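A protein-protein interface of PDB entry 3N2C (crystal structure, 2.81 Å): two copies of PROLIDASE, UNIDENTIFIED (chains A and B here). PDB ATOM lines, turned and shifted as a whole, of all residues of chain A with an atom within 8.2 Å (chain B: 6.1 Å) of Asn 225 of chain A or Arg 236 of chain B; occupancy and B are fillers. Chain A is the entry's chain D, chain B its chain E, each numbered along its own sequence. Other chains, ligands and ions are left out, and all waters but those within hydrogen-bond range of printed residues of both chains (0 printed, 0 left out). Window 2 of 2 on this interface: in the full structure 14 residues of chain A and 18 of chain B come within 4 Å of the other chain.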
ATOM      1  N   ILE A 182       9.037 -33.857  23.573  1.00  0.00           N
ATOM      2  CA  ILE A 182       8.040 -32.863  23.938  1.00  0.00           C
ATOM      3  C   ILE A 182       6.665 -33.496  24.196  1.00  0.00           C
ATOM      4  O   ILE A 182       5.994 -33.154  25.181  1.00  0.00           O
ATOM      5  CB  ILE A 182       8.018 -31.696  22.916  1.00  0.00           C
ATOM      6  CG1 ILE A 182       8.901 -30.557  23.437  1.00  0.00           C
ATOM      7  CG2 ILE A 182       6.607 -31.175  22.662  1.00  0.00           C
ATOM      8  CD1 ILE A 182       9.610 -29.761  22.363  1.00  0.00           C
ATOM      9  N   THR A 187       9.850 -30.218  29.462  1.00  0.00           N
ATOM     10  CA  THR A 187       9.626 -28.779  29.589  1.00  0.00           C
ATOM     11  C   THR A 187      10.746 -27.953  28.958  1.00  0.00           C
ATOM     12  O   THR A 187      10.556 -26.786  28.637  1.00  0.00           O
ATOM     13  CB  THR A 187       9.440 -28.368  31.054  1.00  0.00           C
ATOM     14  OG1 THR A 187      10.544 -28.846  31.828  1.00  0.00           O
ATOM     15  CG2 THR A 187       8.152 -28.946  31.607  1.00  0.00           C
ATOM     16  N   GLN A 188      11.914 -28.563  28.801  1.00  0.00           N
ATOM     17  CA  GLN A 188      13.000 -27.998  28.000  1.00  0.00           C
ATOM     18  C   GLN A 188      13.786 -29.138  27.358  1.00  0.00           C
ATOM     19  O   GLN A 188      13.645 -30.291  27.759  1.00  0.00           O
ATOM     20  CB  GLN A 188      13.914 -27.095  28.836  1.00  0.00           C
ATOM     21  CG  GLN A 188      14.781 -27.816  29.855  1.00  0.00           C
ATOM     22  CD  GLN A 188      14.053 -28.116  31.146  1.00  0.00           C
ATOM     23  OE1 GLN A 188      13.201 -27.345  31.589  1.00  0.00           O
ATOM     24  NE2 GLN A 188      14.389 -29.241  31.763  1.00  0.00           N
ATOM     25  N   VAL A 218      16.925 -26.380  18.195  1.00  0.00           N
ATOM     26  CA  VAL A 218      16.579 -25.042  18.685  1.00  0.00           C
ATOM     27  C   VAL A 218      15.225 -24.601  18.148  1.00  0.00           C
ATOM     28  O   VAL A 218      14.367 -24.167  18.917  1.00  0.00           O
ATOM     29  CB  VAL A 218      17.700 -24.006  18.359  1.00  0.00           C
ATOM     30  CG1 VAL A 218      17.186 -22.567  18.398  1.00  0.00           C
ATOM     31  CG2 VAL A 218      18.883 -24.179  19.316  1.00  0.00           C
ATOM     32  N   ASP A 219      15.018 -24.775  16.846  1.00  0.00           N
ATOM     33  CA  ASP A 219      13.797 -24.324  16.211  1.00  0.00           C
ATOM     34  C   ASP A 219      12.602 -25.185  16.566  1.00  0.00           C
ATOM     35  O   ASP A 219      11.476 -24.695  16.583  1.00  0.00           O
ATOM     36  CB  ASP A 219      13.971 -24.223  14.700  1.00  0.00           C
ATOM     37  CG  ASP A 219      14.796 -23.015  14.290  1.00  0.00           C
ATOM     38  OD1 ASP A 219      15.775 -22.682  14.993  1.00  0.00           O
ATOM     39  OD2 ASP A 219      14.468 -22.393  13.256  1.00  0.00           O
ATOM     40  N   GLU A 220      12.843 -26.458  16.867  1.00  0.00           N
ATOM     41  CA  GLU A 220      11.758 -27.349  17.271  1.00  0.00           C
ATOM     42  C   GLU A 220      11.425 -27.175  18.736  1.00  0.00           C
ATOM     43  O   GLU A 220      10.292 -27.432  19.158  1.00  0.00           O
ATOM     44  CB  GLU A 220      12.089 -28.803  16.964  1.00  0.00           C
ATOM     45  CG  GLU A 220      11.801 -29.193  15.531  1.00  0.00           C
ATOM     46  CD  GLU A 220      10.340 -29.041  15.152  1.00  0.00           C
ATOM     47  OE1 GLU A 220       9.476 -29.591  15.868  1.00  0.00           O
ATOM     48  OE2 GLU A 220      10.056 -28.377  14.132  1.00  0.00           O
ATOM     49  N   ALA A 221      12.412 -26.732  19.509  1.00  0.00           N
ATOM     50  CA  ALA A 221      12.186 -26.370  20.896  1.00  0.00           C
ATOM     51  C   ALA A 221      11.390 -25.074  20.947  1.00  0.00           C
ATOM     52  O   ALA A 221      10.341 -25.021  21.584  1.00  0.00           O
ATOM     53  CB  ALA A 221      13.496 -26.235  21.643  1.00  0.00           C
ATOM     54  N   GLU A 222      11.872 -24.052  20.236  1.00  0.00           N
ATOM     55  CA  GLU A 222      11.209 -22.748  20.172  1.00  0.00           C
ATOM     56  C   GLU A 222       9.774 -22.837  19.658  1.00  0.00           C
ATOM     57  O   GLU A 222       8.914 -22.067  20.084  1.00  0.00           O
ATOM     58  CB  GLU A 222      12.004 -21.771  19.297  1.00  0.00           C
ATOM     59  CG  GLU A 222      13.217 -21.134  19.979  1.00  0.00           C
ATOM     60  CD  GLU A 222      13.979 -20.173  19.067  1.00  0.00           C
ATOM     61  OE1 GLU A 222      13.520 -19.921  17.928  1.00  0.00           O
ATOM     62  OE2 GLU A 222      15.042 -19.664  19.495  1.00  0.00           O
ATOM     63  N   ALA A 223       9.518 -23.783  18.754  1.00  0.00           N
ATOM     64  CA  ALA A 223       8.178 -23.962  18.206  1.00  0.00           C
ATOM     65  C   ALA A 223       7.214 -24.513  19.238  1.00  0.00           C
ATOM     66  O   ALA A 223       6.020 -24.331  19.090  1.00  0.00           O
ATOM     67  CB  ALA A 223       8.192 -24.846  16.969  1.00  0.00           C
ATOM     68  N   ALA A 224       7.728 -25.179  20.273  1.00  0.00           N
ATOM     69  CA  ALA A 224       6.890 -25.659  21.376  1.00  0.00           C
ATOM     70  C   ALA A 224       7.000 -24.754  22.607  1.00  0.00           C
ATOM     71  O   ALA A 224       6.851 -25.207  23.746  1.00  0.00           O
ATOM     72  CB  ALA A 224       7.233 -27.081  21.720  1.00  0.00           C
ATOM     73  N   ASN A 225       7.254 -23.470  22.343  1.00  0.00           N
ATOM     74  CA  ASN A 225       7.414 -22.415  23.353  1.00  0.00           C
ATOM     75  C   ASN A 225       8.335 -22.749  24.527  1.00  0.00           C
ATOM     76  O   ASN A 225       7.995 -22.510  25.685  1.00  0.00           O
ATOM     77  CB  ASN A 225       6.053 -21.882  23.808  1.00  0.00           C
ATOM     78  CG  ASN A 225       5.335 -21.120  22.706  1.00  0.00           C
ATOM     79  OD1 ASN A 225       5.842 -20.119  22.192  1.00  0.00           O
ATOM     80  ND2 ASN A 225       4.152 -21.592  22.335  1.00  0.00           N
ATOM     81  N   THR A 226       9.501 -23.301  24.200  1.00  0.00           N
ATOM     82  CA  THR A 226      10.534 -23.617  25.184  1.00  0.00           C
ATOM     83  C   THR A 226      11.926 -23.282  24.615  1.00  0.00           C
ATOM     84  O   THR A 226      12.026 -22.501  23.670  1.00  0.00           O
ATOM     85  CB  THR A 226      10.397 -25.076  25.729  1.00  0.00           C
ATOM     86  OG1 THR A 226      11.313 -25.283  26.810  1.00  0.00           O
ATOM     87  CG2 THR A 226      10.633 -26.123  24.644  1.00  0.00           C
ATOM     88  N   TYR A 227      12.982 -23.860  25.192  1.00  0.00           N
ATOM     89  CA  TYR A 227      14.364 -23.514  24.860  1.00  0.00           C
ATOM     90  C   TYR A 227      15.287 -24.727  24.891  1.00  0.00           C
ATOM     91  O   TYR A 227      14.876 -25.816  25.277  1.00  0.00           O
ATOM     92  CB  TYR A 227      14.886 -22.446  25.831  1.00  0.00           C
ATOM     93  CG  TYR A 227      15.064 -22.930  27.261  1.00  0.00           C
ATOM     94  CD1 TYR A 227      16.322 -23.267  27.754  1.00  0.00           C
ATOM     95  CD2 TYR A 227      13.975 -23.037  28.122  1.00  0.00           C
ATOM     96  CE1 TYR A 227      16.483 -23.708  29.059  1.00  0.00           C
ATOM     97  CE2 TYR A 227      14.129 -23.475  29.423  1.00  0.00           C
ATOM     98  CZ  TYR A 227      15.380 -23.811  29.887  1.00  0.00           C
ATOM     99  OH  TYR A 227      15.514 -24.248  31.184  1.00  0.00           O
ATOM    100  N   ASN A 361      11.910 -19.997  33.101  1.00  0.00           N
ATOM    101  CA  ASN A 361      10.835 -19.098  32.638  1.00  0.00           C
ATOM    102  C   ASN A 361       9.737 -18.790  33.664  1.00  0.00           C
ATOM    103  O   ASN A 361       8.567 -18.601  33.310  1.00  0.00           O
ATOM    104  CB  ASN A 361      10.250 -19.560  31.298  1.00  0.00           C
ATOM    105  CG  ASN A 361      11.175 -19.280  30.130  1.00  0.00           C
ATOM    106  OD1 ASN A 361      11.666 -20.201  29.476  1.00  0.00           O
ATOM    107  ND2 ASN A 361      11.414 -18.001  29.857  1.00  0.00           N
ATOM    108  N   ALA B 205      -1.221 -22.435  21.565  1.00  0.00           N
ATOM    109  CA  ALA B 205      -0.289 -21.323  21.313  1.00  0.00           C
ATOM    110  C   ALA B 205       0.914 -21.686  20.442  1.00  0.00           C
ATOM    111  O   ALA B 205       1.412 -20.846  19.687  1.00  0.00           O
ATOM    112  CB  ALA B 205       0.180 -20.703  22.635  1.00  0.00           C
ATOM    113  N   ASN B 206       1.380 -22.928  20.543  1.00  0.00           N
ATOM    114  CA  ASN B 206       2.534 -23.336  19.759  1.00  0.00           C
ATOM    115  C   ASN B 206       2.238 -23.779  18.321  1.00  0.00           C
ATOM    116  O   ASN B 206       1.160 -24.293  18.024  1.00  0.00           O
ATOM    117  CB  ASN B 206       3.439 -24.329  20.514  1.00  0.00           C
ATOM    118  CG  ASN B 206       2.688 -25.434  21.227  1.00  0.00           C
ATOM    119  OD1 ASN B 206       2.986 -25.728  22.385  1.00  0.00           O
ATOM    120  ND2 ASN B 206       1.752 -26.084  20.537  1.00  0.00           N
ATOM    121  N   THR B 207       3.218 -23.548  17.446  1.00  0.00           N
ATOM    122  CA  THR B 207       3.147 -23.873  16.024  1.00  0.00           C
ATOM    123  C   THR B 207       3.588 -25.314  15.744  1.00  0.00           C
ATOM    124  O   THR B 207       4.273 -25.936  16.558  1.00  0.00           O
ATOM    125  CB  THR B 207       4.061 -22.943  15.195  1.00  0.00           C
ATOM    126  OG1 THR B 207       5.432 -23.271  15.448  1.00  0.00           O
ATOM    127  CG2 THR B 207       3.818 -21.480  15.534  1.00  0.00           C
ATOM    128  N   THR B 234      -3.359 -19.086  16.054  1.00  0.00           N
ATOM    129  CA  THR B 234      -2.640 -17.873  16.425  1.00  0.00           C
ATOM    130  C   THR B 234      -2.099 -17.179  15.182  1.00  0.00           C
ATOM    131  O   THR B 234      -1.824 -17.828  14.179  1.00  0.00           O
ATOM    132  CB  THR B 234      -1.473 -18.197  17.384  1.00  0.00           C
ATOM    133  OG1 THR B 234      -0.700 -19.273  16.843  1.00  0.00           O
ATOM    134  CG2 THR B 234      -1.992 -18.625  18.745  1.00  0.00           C
ATOM    135  N   GLY B 235      -1.958 -15.858  15.257  1.00  0.00           N
ATOM    136  CA  GLY B 235      -1.437 -15.058  14.150  1.00  0.00           C
ATOM    137  C   GLY B 235       0.002 -15.390  13.807  1.00  0.00           C
ATOM    138  O   GLY B 235       0.411 -15.249  12.655  1.00  0.00           O
ATOM    139  N   ARG B 236       0.761 -15.829  14.815  1.00  0.00           N
ATOM    140  CA  ARG B 236       2.131 -16.315  14.634  1.00  0.00           C
ATOM    141  C   ARG B 236       2.154 -17.543  13.727  1.00  0.00           C
ATOM    142  O   ARG B 236       2.937 -17.594  12.787  1.00  0.00           O
ATOM    143  CB  ARG B 236       2.783 -16.629  15.987  1.00  0.00           C
ATOM    144  CG  ARG B 236       4.206 -17.208  15.921  1.00  0.00           C
ATOM    145  CD  ARG B 236       4.737 -17.468  17.327  1.00  0.00           C
ATOM    146  NE  ARG B 236       5.664 -18.598  17.390  1.00  0.00           N
ATOM    147  CZ  ARG B 236       5.896 -19.329  18.484  1.00  0.00           C
ATOM    148  NH1 ARG B 236       6.758 -20.334  18.440  1.00  0.00           N
ATOM    149  NH2 ARG B 236       5.264 -19.068  19.623  1.00  0.00           N
ATOM    150  N   ALA B 237       1.274 -18.506  14.004  1.00  0.00           N
ATOM    151  CA  ALA B 237       1.172 -19.732  13.211  1.00  0.00           C
ATOM    152  C   ALA B 237       0.559 -19.484  11.832  1.00  0.00           C
ATOM    153  O   ALA B 237       0.921 -20.150  10.861  1.00  0.00           O
ATOM    154  CB  ALA B 237       0.377 -20.791  13.964  1.00  0.00           C
ATOM    155  N   ILE B 238      -0.363 -18.527  11.762  1.00  0.00           N
ATOM    156  CA  ILE B 238      -1.023 -18.157  10.513  1.00  0.00           C
ATOM    157  C   ILE B 238      -0.041 -17.482   9.557  1.00  0.00           C
ATOM    158  O   ILE B 238       0.009 -17.832   8.372  1.00  0.00           O
ATOM    159  CB  ILE B 238      -2.258 -17.254  10.766  1.00  0.00           C
ATOM    160  CG1 ILE B 238      -3.433 -18.099  11.237  1.00  0.00           C
ATOM    161  CG2 ILE B 238      -2.682 -16.515   9.504  1.00  0.00           C
ATOM    162  CD1 ILE B 238      -4.471 -17.338  11.987  1.00  0.00           C
ATOM    163  N   ALA B 239       0.751 -16.548  10.086  1.00  0.00           N
ATOM    164  CA  ALA B 239       1.675 -15.759   9.274  1.00  0.00           C
ATOM    165  C   ALA B 239       2.738 -16.610   8.576  1.00  0.00           C
ATOM    166  O   ALA B 239       2.977 -16.435   7.381  1.00  0.00           O
ATOM    167  CB  ALA B 239       2.322 -14.674  10.104  1.00  0.00           C
ATOM    168  N   ARG B 240       3.344 -17.540   9.314  1.00  0.00           N
ATOM    169  CA  ARG B 240       4.403 -18.392   8.763  1.00  0.00           C
ATOM    170  C   ARG B 240       3.874 -19.385   7.738  1.00  0.00           C
ATOM    171  O   ARG B 240       4.552 -19.671   6.749  1.00  0.00           O
ATOM    172  CB  ARG B 240       5.194 -19.118   9.858  1.00  0.00           C
ATOM    173  CG  ARG B 240       4.347 -19.738  10.930  1.00  0.00           C
ATOM    174  CD  ARG B 240       4.602 -21.204  11.053  1.00  0.00           C
ATOM    175  NE  ARG B 240       5.934 -21.488  11.564  1.00  0.00           N
ATOM    176  CZ  ARG B 240       6.417 -22.716  11.695  1.00  0.00           C
ATOM    177  NH1 ARG B 240       5.675 -23.758  11.347  1.00  0.00           N
ATOM    178  NH2 ARG B 240       7.638 -22.904  12.169  1.00  0.00           N
ATOM    179  N   ALA B 241       2.665 -19.890   7.973  1.00  0.00           N
ATOM    180  CA  ALA B 241       2.020 -20.811   7.048  1.00  0.00           C
ATOM    181  C   ALA B 241       1.747 -20.125   5.715  1.00  0.00           C
ATOM    182  O   ALA B 241       2.048 -20.681   4.660  1.00  0.00           O
ATOM    183  CB  ALA B 241       0.736 -21.350   7.643  1.00  0.00           C
ATOM    184  N   ARG B 243       3.140 -17.340   4.583  1.00  0.00           N
ATOM    185  CA  ARG B 243       4.449 -16.999   4.016  1.00  0.00           C
ATOM    186  C   ARG B 243       5.115 -18.163   3.279  1.00  0.00           C
ATOM    187  O   ARG B 243       5.839 -17.950   2.307  1.00  0.00           O
ATOM    188  CB  ARG B 243       5.390 -16.458   5.091  1.00  0.00           C
ATOM    189  CG  ARG B 243       5.640 -14.976   4.982  1.00  0.00           C
ATOM    190  CD  ARG B 243       6.702 -14.517   5.962  1.00  0.00           C
ATOM    191  NE  ARG B 243       6.132 -13.745   7.066  1.00  0.00           N
ATOM    192  CZ  ARG B 243       5.918 -14.215   8.293  1.00  0.00           C
ATOM    193  NH1 ARG B 243       6.229 -15.470   8.598  1.00  0.00           N
ATOM    194  NH2 ARG B 243       5.401 -13.421   9.223  1.00  0.00           N
ATOM    195  N   LEU B 254      -7.517 -16.837  16.419  1.00  0.00           N
ATOM    196  CA  LEU B 254      -6.699 -15.930  17.222  1.00  0.00           C
ATOM    197  C   LEU B 254      -5.779 -15.014  16.402  1.00  0.00           C
ATOM    198  O   LEU B 254      -4.650 -14.725  16.814  1.00  0.00           O
ATOM    199  CB  LEU B 254      -5.916 -16.719  18.285  1.00  0.00           C
ATOM    200  CG  LEU B 254      -6.717 -17.625  19.235  1.00  0.00           C
ATOM    201  CD1 LEU B 254      -5.808 -18.245  20.281  1.00  0.00           C
ATOM    202  CD2 LEU B 254      -7.868 -16.881  19.912  1.00  0.00           C
ATOM    203  N   ASP B 256      -4.250 -11.586  14.719  1.00  0.00           N
ATOM    204  CA  ASP B 256      -4.079 -10.149  14.887  1.00  0.00           C
ATOM    205  C   ASP B 256      -4.328  -9.521  13.521  1.00  0.00           C
ATOM    206  O   ASP B 256      -4.373 -10.236  12.518  1.00  0.00           O
ATOM    207  CB  ASP B 256      -2.675  -9.823  15.409  1.00  0.00           C
ATOM    208  CG  ASP B 256      -1.625 -10.812  14.933  1.00  0.00           C
ATOM    209  OD1 ASP B 256      -1.174 -10.695  13.775  1.00  0.00           O
ATOM    210  OD2 ASP B 256      -1.244 -11.701  15.727  1.00  0.00           O
ATOM    211  N   ALA B 259      -1.467 -10.166  10.799  1.00  0.00           N
ATOM    212  CA  ALA B 259      -1.483 -11.416  10.039  1.00  0.00           C
ATOM    213  C   ALA B 259      -2.576 -11.424   8.976  1.00  0.00           C
ATOM    214  O   ALA B 259      -2.373 -11.942   7.879  1.00  0.00           O
ATOM    215  CB  ALA B 259      -1.640 -12.605  10.969  1.00  0.00           C
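No position is printed for both chains.
Of the 14 printed residues of chain A, 4 touch a printed residue of chain B.
Printed residues of chain A that touch a printed residue of chain B: Glu 222, Ala 223, Ala 224 and Asn 225.
Hydrophobic or aromatic side chains of chain A within 4 Å of the printed part of chain B: Ala 223.
Among the printed residues, 8 pairs touch across the chains.
The backbone carbonyl oxygen (O) of Ala 223 of chain A is in hydrogen-bond range of the backbone NH (N) of Thr 207 of chain B (3.3 Å).
The side-chain amide oxygen of Asn 225 of chain A is in hydrogen-bond range of the guanidinium group of Arg 236 of chain B (2.8 Å).
The guanidinium group (NH1) of Arg 236 of chain B sits at hydrogen-bond distance from the backbone carbonyl oxygen (O) of Glu 222 of chain A.
Among the printed residues, pairs that only touch across the chains: Ala 223 of chain A with Asn 206 of chain B, Asn 225 of chain A with Asn 206 of chain B, Asn 225 of chain A with Ala 205 of chain B, Ala 224 of chain A with Asn 206 of chain B and Ala 223 of chain A with Arg 236 of chain B.
Of chain B, only Ala 205, Asn 206 and Arg 236 come within 4 Å of Asn 225 of chain A.
Of chain A, only Glu 222 (3.2 Å), Ala 223 (3.9 Å) and Asn 225 (2.8 Å) come within 4 Å of Arg 236 of chain B.
Gly 235 of chain B touches none of the printed residues of chain A.
No residue of chain A comes within 4 Å of Ala 237 of chain B.
Of the printed residues of chain B, Ala 224 of chain A touches Asn 206 (3.8 Å).
Of the printed residues of chain B, Ala 223 of chain A touches Asn 206 (2.9 Å), Thr 207 (3.3 Å) and Arg 236 (3.9 Å).
Of the printed residues of chain A, Ala 205 of chain B touches Asn 225.
Of the printed residues of chain B, Glu 222 of chain A touches Arg 236.
Of the printed residues of chain A, Asn 206 of chain B touches Ala 223 (2.9 Å), Ala 224 (3.8 Å) and Asn 225 (3.4 Å).
Ile 182 of chain A touches none of the printed residues of chain B.
The nearest residue of chain A that does not touch Arg 236 of chain B is Ala 224 of chain A (5.3 Å).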
